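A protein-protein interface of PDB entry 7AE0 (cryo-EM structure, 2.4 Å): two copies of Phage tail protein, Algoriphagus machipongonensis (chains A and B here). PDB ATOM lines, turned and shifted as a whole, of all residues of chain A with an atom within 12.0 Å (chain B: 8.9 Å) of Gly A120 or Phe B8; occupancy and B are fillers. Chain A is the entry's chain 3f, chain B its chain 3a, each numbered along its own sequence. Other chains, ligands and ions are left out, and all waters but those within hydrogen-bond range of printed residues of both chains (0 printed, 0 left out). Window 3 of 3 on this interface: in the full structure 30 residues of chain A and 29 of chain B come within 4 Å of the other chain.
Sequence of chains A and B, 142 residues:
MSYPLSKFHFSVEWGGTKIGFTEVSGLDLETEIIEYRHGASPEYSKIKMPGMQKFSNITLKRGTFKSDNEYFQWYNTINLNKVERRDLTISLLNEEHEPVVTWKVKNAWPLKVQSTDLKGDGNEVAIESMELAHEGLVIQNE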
ATOM      1  N   THR A  64     -15.433   1.208   4.043  1.00  0.00           N
ATOM      2  CA  THR A  64     -14.756   1.031   2.750  1.00  0.00           C
ATOM      3  C   THR A  64     -15.413  -0.013   1.845  1.00  0.00           C
ATOM      4  O   THR A  64     -15.650  -1.150   2.255  1.00  0.00           O
ATOM      5  CB  THR A  64     -13.281   0.655   2.985  1.00  0.00           C
ATOM      6  OG1 THR A  64     -12.634   1.715   3.685  1.00  0.00           O
ATOM      7  CG2 THR A  64     -12.547   0.442   1.672  1.00  0.00           C
ATOM      8  N   THR A 116      -7.873   3.112   7.434  1.00  0.00           N
ATOM      9  CA  THR A 116      -8.026   2.011   8.391  1.00  0.00           C
ATOM     10  C   THR A 116      -6.713   1.341   8.860  1.00  0.00           C
ATOM     11  O   THR A 116      -5.709   1.327   8.150  1.00  0.00           O
ATOM     12  CB  THR A 116      -8.917   0.940   7.712  1.00  0.00           C
ATOM     13  OG1 THR A 116      -9.486   0.065   8.678  1.00  0.00           O
ATOM     14  CG2 THR A 116      -8.137   0.097   6.683  1.00  0.00           C
ATOM     15  N   ASP A 117      -6.721   0.855  10.091  1.00  0.00           N
ATOM     16  CA  ASP A 117      -5.639   0.032  10.603  1.00  0.00           C
ATOM     17  C   ASP A 117      -5.895  -1.439  10.204  1.00  0.00           C
ATOM     18  O   ASP A 117      -6.985  -1.790   9.813  1.00  0.00           O
ATOM     19  CB  ASP A 117      -5.518   0.231  12.108  1.00  0.00           C
ATOM     20  CG  ASP A 117      -6.811  -0.052  12.848  1.00  0.00           C
ATOM     21  OD1 ASP A 117      -7.902  -0.001  12.253  1.00  0.00           O
ATOM     22  OD2 ASP A 117      -6.743  -0.327  14.049  1.00  0.00           O
ATOM     23  N   LEU A 118      -4.881  -2.282  10.216  1.00  0.00           N
ATOM     24  CA  LEU A 118      -5.056  -3.684   9.869  1.00  0.00           C
ATOM     25  C   LEU A 118      -4.622  -4.571  11.024  1.00  0.00           C
ATOM     26  O   LEU A 118      -3.571  -4.340  11.614  1.00  0.00           O
ATOM     27  CB  LEU A 118      -4.239  -3.976   8.611  1.00  0.00           C
ATOM     28  CG  LEU A 118      -4.558  -3.091   7.375  1.00  0.00           C
ATOM     29  CD1 LEU A 118      -3.566  -3.363   6.283  1.00  0.00           C
ATOM     30  CD2 LEU A 118      -5.962  -3.355   6.869  1.00  0.00           C
ATOM     31  N   LYS A 119      -5.420  -5.589  11.348  1.00  0.00           N
ATOM     32  CA  LYS A 119      -5.085  -6.508  12.440  1.00  0.00           C
ATOM     33  C   LYS A 119      -5.367  -7.960  12.073  1.00  0.00           C
ATOM     34  O   LYS A 119      -6.409  -8.269  11.500  1.00  0.00           O
ATOM     35  CB  LYS A 119      -5.888  -6.139  13.680  1.00  0.00           C
ATOM     36  CG  LYS A 119      -5.558  -4.802  14.267  1.00  0.00           C
ATOM     37  CD  LYS A 119      -6.337  -4.553  15.527  1.00  0.00           C
ATOM     38  CE  LYS A 119      -6.009  -3.188  16.097  1.00  0.00           C
ATOM     39  NZ  LYS A 119      -6.771  -2.903  17.338  1.00  0.00           N
ATOM     40  N   GLY A 120      -4.455  -8.854  12.473  1.00  0.00           N
ATOM     41  CA  GLY A 120      -4.593 -10.292  12.221  1.00  0.00           C
ATOM     42  C   GLY A 120      -5.840 -10.915  12.827  1.00  0.00           C
ATOM     43  O   GLY A 120      -6.415 -11.850  12.264  1.00  0.00           O
ATOM     44  N   ASP A 121      -6.270 -10.402  13.969  1.00  0.00           N
ATOM     45  CA  ASP A 121      -7.464 -10.839  14.667  1.00  0.00           C
ATOM     46  C   ASP A 121      -8.545  -9.753  14.669  1.00  0.00           C
ATOM     47  O   ASP A 121      -9.465  -9.760  15.495  1.00  0.00           O
ATOM     48  CB  ASP A 121      -7.057 -11.283  16.063  1.00  0.00           C
ATOM     49  CG  ASP A 121      -6.302 -10.215  16.789  1.00  0.00           C
ATOM     50  OD1 ASP A 121      -5.899  -9.246  16.142  1.00  0.00           O
ATOM     51  OD2 ASP A 121      -6.102 -10.338  17.981  1.00  0.00           O
ATOM     52  N   GLY A 122      -8.470  -8.843  13.707  1.00  0.00           N
ATOM     53  CA  GLY A 122      -9.390  -7.732  13.584  1.00  0.00           C
ATOM     54  C   GLY A 122     -10.715  -8.099  12.963  1.00  0.00           C
ATOM     55  O   GLY A 122     -10.995  -7.747  11.817  1.00  0.00           O
ATOM     56  N   ASN A 123     -11.554  -8.783  13.722  1.00  0.00           N
ATOM     57  CA  ASN A 123     -12.853  -9.227  13.222  1.00  0.00           C
ATOM     58  C   ASN A 123     -13.873  -8.087  13.184  1.00  0.00           C
ATOM     59  O   ASN A 123     -14.838  -8.082  13.952  1.00  0.00           O
ATOM     60  CB  ASN A 123     -13.377 -10.355  14.093  1.00  0.00           C
ATOM     61  CG  ASN A 123     -14.562 -11.050  13.499  1.00  0.00           C
ATOM     62  OD1 ASN A 123     -14.681 -11.161  12.283  1.00  0.00           O
ATOM     63  ND2 ASN A 123     -15.449 -11.510  14.339  1.00  0.00           N
ATOM     64  N   GLU A 124     -13.647  -7.125  12.264  1.00  0.00           N
ATOM     65  CA  GLU A 124     -14.552  -5.977  12.117  1.00  0.00           C
ATOM     66  C   GLU A 124     -14.435  -5.263  10.758  1.00  0.00           C
ATOM     67  O   GLU A 124     -13.579  -5.571   9.928  1.00  0.00           O
ATOM     68  CB  GLU A 124     -14.329  -4.960  13.227  1.00  0.00           C
ATOM     69  CG  GLU A 124     -12.912  -4.455  13.361  1.00  0.00           C
ATOM     70  CD  GLU A 124     -12.761  -3.435  14.472  1.00  0.00           C
ATOM     71  OE1 GLU A 124     -13.758  -3.168  15.173  1.00  0.00           O
ATOM     72  OE2 GLU A 124     -11.632  -2.941  14.681  1.00  0.00           O
ATOM     73  N   VAL A 125     -15.333  -4.292  10.553  1.00  0.00           N
ATOM     74  CA  VAL A 125     -15.445  -3.538   9.302  1.00  0.00           C
ATOM     75  C   VAL A 125     -14.365  -2.476   9.188  1.00  0.00           C
ATOM     76  O   VAL A 125     -14.101  -1.734  10.132  1.00  0.00           O
ATOM     77  CB  VAL A 125     -16.825  -2.862   9.191  1.00  0.00           C
ATOM     78  CG1 VAL A 125     -16.917  -1.974   7.938  1.00  0.00           C
ATOM     79  CG2 VAL A 125     -17.886  -3.896   9.150  1.00  0.00           C
ATOM     80  N   ALA A 126     -13.753  -2.384   8.022  1.00  0.00           N
ATOM     81  CA  ALA A 126     -12.770  -1.348   7.762  1.00  0.00           C
ATOM     82  C   ALA A 126     -13.466   0.004   7.534  1.00  0.00           C
ATOM     83  O   ALA A 126     -14.227   0.145   6.573  1.00  0.00           O
ATOM     84  CB  ALA A 126     -11.951  -1.762   6.550  1.00  0.00           C
ATOM     85  N   ILE A 127     -13.224   0.981   8.427  1.00  0.00           N
ATOM     86  CA  ILE A 127     -13.867   2.308   8.386  1.00  0.00           C
ATOM     87  C   ILE A 127     -12.895   3.435   8.052  1.00  0.00           C
ATOM     88  O   ILE A 127     -11.971   3.705   8.815  1.00  0.00           O
ATOM     89  CB  ILE A 127     -14.528   2.675   9.738  1.00  0.00           C
ATOM     90  CG1 ILE A 127     -15.565   1.618  10.200  1.00  0.00           C
ATOM     91  CG2 ILE A 127     -15.163   4.108   9.696  1.00  0.00           C
ATOM     92  CD1 ILE A 127     -16.758   1.407   9.294  1.00  0.00           C
ATOM     93  N   LEU B   5     -15.851  -4.116   3.097  1.00  0.00           N
ATOM     94  CA  LEU B   5     -14.682  -4.971   3.269  1.00  0.00           C
ATOM     95  C   LEU B   5     -14.334  -5.176   4.746  1.00  0.00           C
ATOM     96  O   LEU B   5     -14.507  -4.272   5.566  1.00  0.00           O
ATOM     97  CB  LEU B   5     -13.498  -4.312   2.554  1.00  0.00           C
ATOM     98  CG  LEU B   5     -13.609  -4.099   1.019  1.00  0.00           C
ATOM     99  CD1 LEU B   5     -12.478  -3.213   0.546  1.00  0.00           C
ATOM    100  CD2 LEU B   5     -13.533  -5.427   0.303  1.00  0.00           C
ATOM    101  N   SER B   6     -13.790  -6.353   5.074  1.00  0.00           N
ATOM    102  CA  SER B   6     -13.281  -6.670   6.410  1.00  0.00           C
ATOM    103  C   SER B   6     -11.844  -6.162   6.546  1.00  0.00           C
ATOM    104  O   SER B   6     -11.259  -5.692   5.575  1.00  0.00           O
ATOM    105  CB  SER B   6     -13.351  -8.166   6.678  1.00  0.00           C
ATOM    106  OG  SER B   6     -12.460  -8.870   5.860  1.00  0.00           O
ATOM    107  N   LYS B   7     -11.258  -6.263   7.750  1.00  0.00           N
ATOM    108  CA  LYS B   7      -9.911  -5.706   7.987  1.00  0.00           C
ATOM    109  C   LYS B   7      -8.837  -6.725   8.402  1.00  0.00           C
ATOM    110  O   LYS B   7      -7.772  -6.284   8.862  1.00  0.00           O
ATOM    111  CB  LYS B   7      -9.983  -4.587   9.037  1.00  0.00           C
ATOM    112  CG  LYS B   7     -10.532  -5.009  10.394  1.00  0.00           C
ATOM    113  CD  LYS B   7     -10.631  -3.863  11.379  1.00  0.00           C
ATOM    114  CE  LYS B   7      -9.293  -3.211  11.662  1.00  0.00           C
ATOM    115  NZ  LYS B   7      -9.426  -2.096  12.631  1.00  0.00           N
ATOM    116  N   PHE B   8      -9.043  -8.044   8.236  1.00  0.00           N
ATOM    117  CA  PHE B   8      -8.021  -8.988   8.703  1.00  0.00           C
ATOM    118  C   PHE B   8      -7.199  -9.749   7.650  1.00  0.00           C
ATOM    119  O   PHE B   8      -6.264 -10.456   8.027  1.00  0.00           O
ATOM    120  CB  PHE B   8      -8.649 -10.000   9.670  1.00  0.00           C
ATOM    121  CG  PHE B   8      -9.772 -10.795   9.101  1.00  0.00           C
ATOM    122  CD1 PHE B   8      -9.538 -11.944   8.370  1.00  0.00           C
ATOM    123  CD2 PHE B   8     -11.074 -10.406   9.318  1.00  0.00           C
ATOM    124  CE1 PHE B   8     -10.572 -12.666   7.859  1.00  0.00           C
ATOM    125  CE2 PHE B   8     -12.113 -11.137   8.810  1.00  0.00           C
ATOM    126  CZ  PHE B   8     -11.861 -12.265   8.081  1.00  0.00           C
ATOM    127  N   HIS B   9      -7.492  -9.640   6.367  1.00  0.00           N
ATOM    128  CA  HIS B   9      -6.723 -10.374   5.357  1.00  0.00           C
ATOM    129  C   HIS B   9      -5.920  -9.388   4.498  1.00  0.00           C
ATOM    130  O   HIS B   9      -6.495  -8.637   3.703  1.00  0.00           O
ATOM    131  CB  HIS B   9      -7.689 -11.224   4.536  1.00  0.00           C
ATOM    132  CG  HIS B   9      -7.075 -12.145   3.538  1.00  0.00           C
ATOM    133  ND1 HIS B   9      -7.772 -12.530   2.426  1.00  0.00           N
ATOM    134  CD2 HIS B   9      -5.892 -12.799   3.483  1.00  0.00           C
ATOM    135  CE1 HIS B   9      -7.046 -13.354   1.711  1.00  0.00           C
ATOM    136  NE2 HIS B   9      -5.897 -13.541   2.326  1.00  0.00           N
ATOM    137  N   PHE B  10      -4.600  -9.364   4.691  1.00  0.00           N
ATOM    138  CA  PHE B  10      -3.731  -8.379   4.043  1.00  0.00           C
ATOM    139  C   PHE B  10      -2.291  -8.873   3.926  1.00  0.00           C
ATOM    140  O   PHE B  10      -1.902  -9.834   4.583  1.00  0.00           O
ATOM    141  CB  PHE B  10      -3.770  -7.051   4.823  1.00  0.00           C
ATOM    142  CG  PHE B  10      -3.287  -7.152   6.258  1.00  0.00           C
ATOM    143  CD1 PHE B  10      -1.962  -6.893   6.590  1.00  0.00           C
ATOM    144  CD2 PHE B  10      -4.161  -7.504   7.274  1.00  0.00           C
ATOM    145  CE1 PHE B  10      -1.528  -6.998   7.888  1.00  0.00           C
ATOM    146  CE2 PHE B  10      -3.727  -7.607   8.572  1.00  0.00           C
ATOM    147  CZ  PHE B  10      -2.405  -7.354   8.883  1.00  0.00           C
ATOM    148  N   SER B  11      -1.482  -8.169   3.121  1.00  0.00           N
ATOM    149  CA  SER B  11      -0.051  -8.473   3.006  1.00  0.00           C
ATOM    150  C   SER B  11       0.833  -7.232   2.835  1.00  0.00           C
ATOM    151  O   SER B  11       0.395  -6.191   2.336  1.00  0.00           O
ATOM    152  CB  SER B  11       0.196  -9.401   1.842  1.00  0.00           C
ATOM    153  OG  SER B  11      -0.119  -8.778   0.631  1.00  0.00           O
ATOM    154  N   GLY B  20       3.983 -11.578   6.093  1.00  0.00           N
ATOM    155  CA  GLY B  20       2.956 -11.654   7.118  1.00  0.00           C
ATOM    156  C   GLY B  20       3.248 -10.782   8.330  1.00  0.00           C
ATOM    157  O   GLY B  20       4.326 -10.850   8.921  1.00  0.00           O
ATOM    158  N   PHE B  21       2.255  -9.999   8.720  1.00  0.00           N
ATOM    159  CA  PHE B  21       2.344  -9.093   9.858  1.00  0.00           C
ATOM    160  C   PHE B  21       1.134  -9.229  10.756  1.00  0.00           C
ATOM    161  O   PHE B  21       0.062  -9.639  10.322  1.00  0.00           O
ATOM    162  CB  PHE B  21       2.513  -7.637   9.392  1.00  0.00           C
ATOM    163  CG  PHE B  21       3.866  -7.352   8.809  1.00  0.00           C
ATOM    164  CD1 PHE B  21       4.206  -7.719   7.526  1.00  0.00           C
ATOM    165  CD2 PHE B  21       4.808  -6.697   9.561  1.00  0.00           C
ATOM    166  CE1 PHE B  21       5.453  -7.459   7.029  1.00  0.00           C
ATOM    167  CE2 PHE B  21       6.055  -6.429   9.050  1.00  0.00           C
ATOM    168  CZ  PHE B  21       6.372  -6.813   7.791  1.00  0.00           C
ATOM    169  N   THR B  22       1.330  -8.891  12.017  1.00  0.00           N
ATOM    170  CA  THR B  22       0.269  -8.865  13.009  1.00  0.00           C
ATOM    171  C   THR B  22      -0.522  -7.570  12.961  1.00  0.00           C
ATOM    172  O   THR B  22      -1.751  -7.579  13.069  1.00  0.00           O
ATOM    173  CB  THR B  22       0.825  -9.151  14.427  1.00  0.00           C
ATOM    174  OG1 THR B  22       1.444 -10.449  14.484  1.00  0.00           O
ATOM    175  CG2 THR B  22      -0.231  -9.057  15.452  1.00  0.00           C
ATOM    176  N   GLU B  23       0.173  -6.451  12.805  1.00  0.00           N
ATOM    177  CA  GLU B  23      -0.484  -5.152  12.835  1.00  0.00           C
ATOM    178  C   GLU B  23       0.187  -4.110  11.942  1.00  0.00           C
ATOM    179  O   GLU B  23       1.415  -4.046  11.853  1.00  0.00           O
ATOM    180  CB  GLU B  23      -0.538  -4.633  14.271  1.00  0.00           C
ATOM    181  CG  GLU B  23      -1.276  -3.319  14.459  1.00  0.00           C
ATOM    182  CD  GLU B  23      -1.315  -2.871  15.893  1.00  0.00           C
ATOM    183  OE1 GLU B  23      -0.970  -3.641  16.775  1.00  0.00           O
ATOM    184  OE2 GLU B  23      -1.675  -1.737  16.132  1.00  0.00           O
ATOM    185  N   VAL B  24      -0.638  -3.306  11.262  1.00  0.00           N
ATOM    186  CA  VAL B  24      -0.194  -2.187  10.423  1.00  0.00           C
ATOM    187  C   VAL B  24      -0.989  -0.918  10.772  1.00  0.00           C
ATOM    188  O   VAL B  24      -2.221  -0.944  10.737  1.00  0.00           O
ATOM    189  CB  VAL B  24      -0.386  -2.506   8.921  1.00  0.00           C
ATOM    190  CG1 VAL B  24       0.072  -1.321   8.046  1.00  0.00           C
ATOM    191  CG2 VAL B  24       0.353  -3.781   8.542  1.00  0.00           C
ATOM    192  N   LYS B  61       4.072  -4.414  13.108  1.00  0.00           N
ATOM    193  CA  LYS B  61       4.282  -5.345  14.236  1.00  0.00           C
ATOM    194  C   LYS B  61       4.271  -6.801  13.756  1.00  0.00           C
ATOM    195  O   LYS B  61       3.401  -7.159  12.953  1.00  0.00           O
ATOM    196  CB  LYS B  61       3.199  -5.135  15.307  1.00  0.00           C
ATOM    197  CG  LYS B  61       3.196  -3.758  15.961  1.00  0.00           C
ATOM    198  CD  LYS B  61       2.165  -3.625  17.061  1.00  0.00           C
ATOM    199  CE  LYS B  61       2.181  -2.261  17.725  1.00  0.00           C
ATOM    200  NZ  LYS B  61       1.174  -2.168  18.811  1.00  0.00           N
ATOM    201  N   SER B  91      -1.195  -4.071   0.901  1.00  0.00           N
ATOM    202  CA  SER B  91      -2.402  -4.450   0.174  1.00  0.00           C
ATOM    203  C   SER B  91      -3.450  -5.276   0.928  1.00  0.00           C
ATOM    204  O   SER B  91      -3.144  -6.252   1.617  1.00  0.00           O
ATOM    205  CB  SER B  91      -1.968  -5.188  -1.073  1.00  0.00           C
ATOM    206  OG  SER B  91      -3.054  -5.689  -1.769  1.00  0.00           O
ATOM    207  N   LEU B  92      -4.706  -4.857   0.782  1.00  0.00           N
ATOM    208  CA  LEU B  92      -5.885  -5.521   1.350  1.00  0.00           C
ATOM    209  C   LEU B  92      -6.408  -6.531   0.315  1.00  0.00           C
ATOM    210  O   LEU B  92      -6.709  -6.181  -0.810  1.00  0.00           O
ATOM    211  CB  LEU B  92      -6.946  -4.475   1.732  1.00  0.00           C
ATOM    212  CG  LEU B  92      -8.072  -4.767   2.735  1.00  0.00           C
ATOM    213  CD1 LEU B  92      -8.752  -3.510   3.220  1.00  0.00           C
ATOM    214  CD2 LEU B  92      -9.103  -5.698   2.143  1.00  0.00           C
ATOM    215  N   LEU B  93      -6.574  -7.776   0.715  1.00  0.00           N
ATOM    216  CA  LEU B  93      -6.861  -8.889  -0.194  1.00  0.00           C
ATOM    217  C   LEU B  93      -8.304  -9.418  -0.246  1.00  0.00           C
ATOM    218  O   LEU B  93      -9.049  -9.351   0.732  1.00  0.00           O
ATOM    219  CB  LEU B  93      -5.955 -10.045   0.201  1.00  0.00           C
ATOM    220  CG  LEU B  93      -4.442  -9.760   0.207  1.00  0.00           C
ATOM    221  CD1 LEU B  93      -3.734 -10.948   0.764  1.00  0.00           C
ATOM    222  CD2 LEU B  93      -3.942  -9.450  -1.186  1.00  0.00           C
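The side-chain amino group (NZ) of Lys B7 is in salt-bridge range of the side-chain carboxylate (OE2) of Glu A124. The backbone NH (N) of Leu B5 lies within hydrogen-bond range of the backbone carbonyl oxygen (O) of Thr A64. The backbone carbonyl oxygen (O) of Leu B5 is in hydrogen-bond range of the backbone NH (N) of Ala A126 (3.2 Å). The backbone NH (N) of Lys A119 lies within hydrogen-bond range of the backbone carbonyl oxygen (O) of Lys B7 (3.5 Å). The backbone carbonyl oxygen (O) of Val B24 lies within hydrogen-bond range of the backbone NH (N) of Leu A118 (3.0 Å). N of Gly A120 is in hydrogen-bond range of O of Thr B22, 3.0 Å away. NZ of Lys B7 is in salt-bridge range of OD1 of Asp A117, at 2.6 Å.
NZ of Lys B61 is in salt-bridge range of OE1 of Glu B23. The backbone NH (N) of Thr A64 lies within hydrogen-bond range of the backbone carbonyl oxygen (O) of Ala A126, 3.0 Å away. The backbone carbonyl oxygen of Lys B61 sits at hydrogen-bond distance from the backbone NH of Thr B22 (2.9 Å).
CA of Asp A117 touches O of Val B24, at 3.6 Å. Phe B10 touches Leu A118 (CE2 to CB, 3.7 Å). O of Leu A118 touches O of Thr B22, 3.99 Å away. O of Lys A119 touches CA of Phe B8 (3.3 Å). N of Lys A119 touches CE2 of Phe B10, at 3.8 Å. O of Thr B22 touches CA of Lys A119 (3.6 Å). Gly A120 touches Phe B8 (O to CB, 3.9 Å). O of Gly A122 touches CG of Lys B7, at 3.1 Å. CD2 of Phe B8 touches O of Gly A122, at 3.6 Å. O of Glu A124 touches CA of Ser B6 (3.7 Å).
Gly A120 touches two residues of chain B. Of chain A, only Lys A119, Gly A120 and Gly A122 come within 4 Å of Phe B8. Of chain B, only Lys B7 (3.1 Å) and Phe B8 (3.6 Å) come within 4 Å of Gly A122. Ser B6 touches just one residue of chain A: Glu A124 (3.7 Å). No residue of chain A comes within 4 Å of His B9. Phe B10 touches just these residues of chain A: Leu A118 and Lys A119. Printed residues of chain B within 4 Å of Asp A117: Lys B7 and Val B24. Of the printed residues of chain B, Val A125 touches Leu B5. Thr A116 touches none of the printed residues of chain B. Ser B91 touches none of the printed residues of chain A. The nearest residue of chain B that does not touch Gly A120 is Phe B10 (4.2 Å). The nearest printed residue of chain A that does not touch Thr B22 is Asp A121 (5.4 Å).
Hydrophobic or aromatic side chains of chain A that line the printed part of chain B: Leu A118 and Ala A126. Printed residues of chain B that touch a printed residue of chain A: Leu B5, Ser B6, Lys B7, Phe B8, Phe B10, Thr B22, Glu B23 and Val B24. Among the printed residues, 20 pairs touch across the chains.
No position is printed for both chains. Of the 20 pairs that touch across the chains among the printed residues, none has its exchanged pair printed and touching as well.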
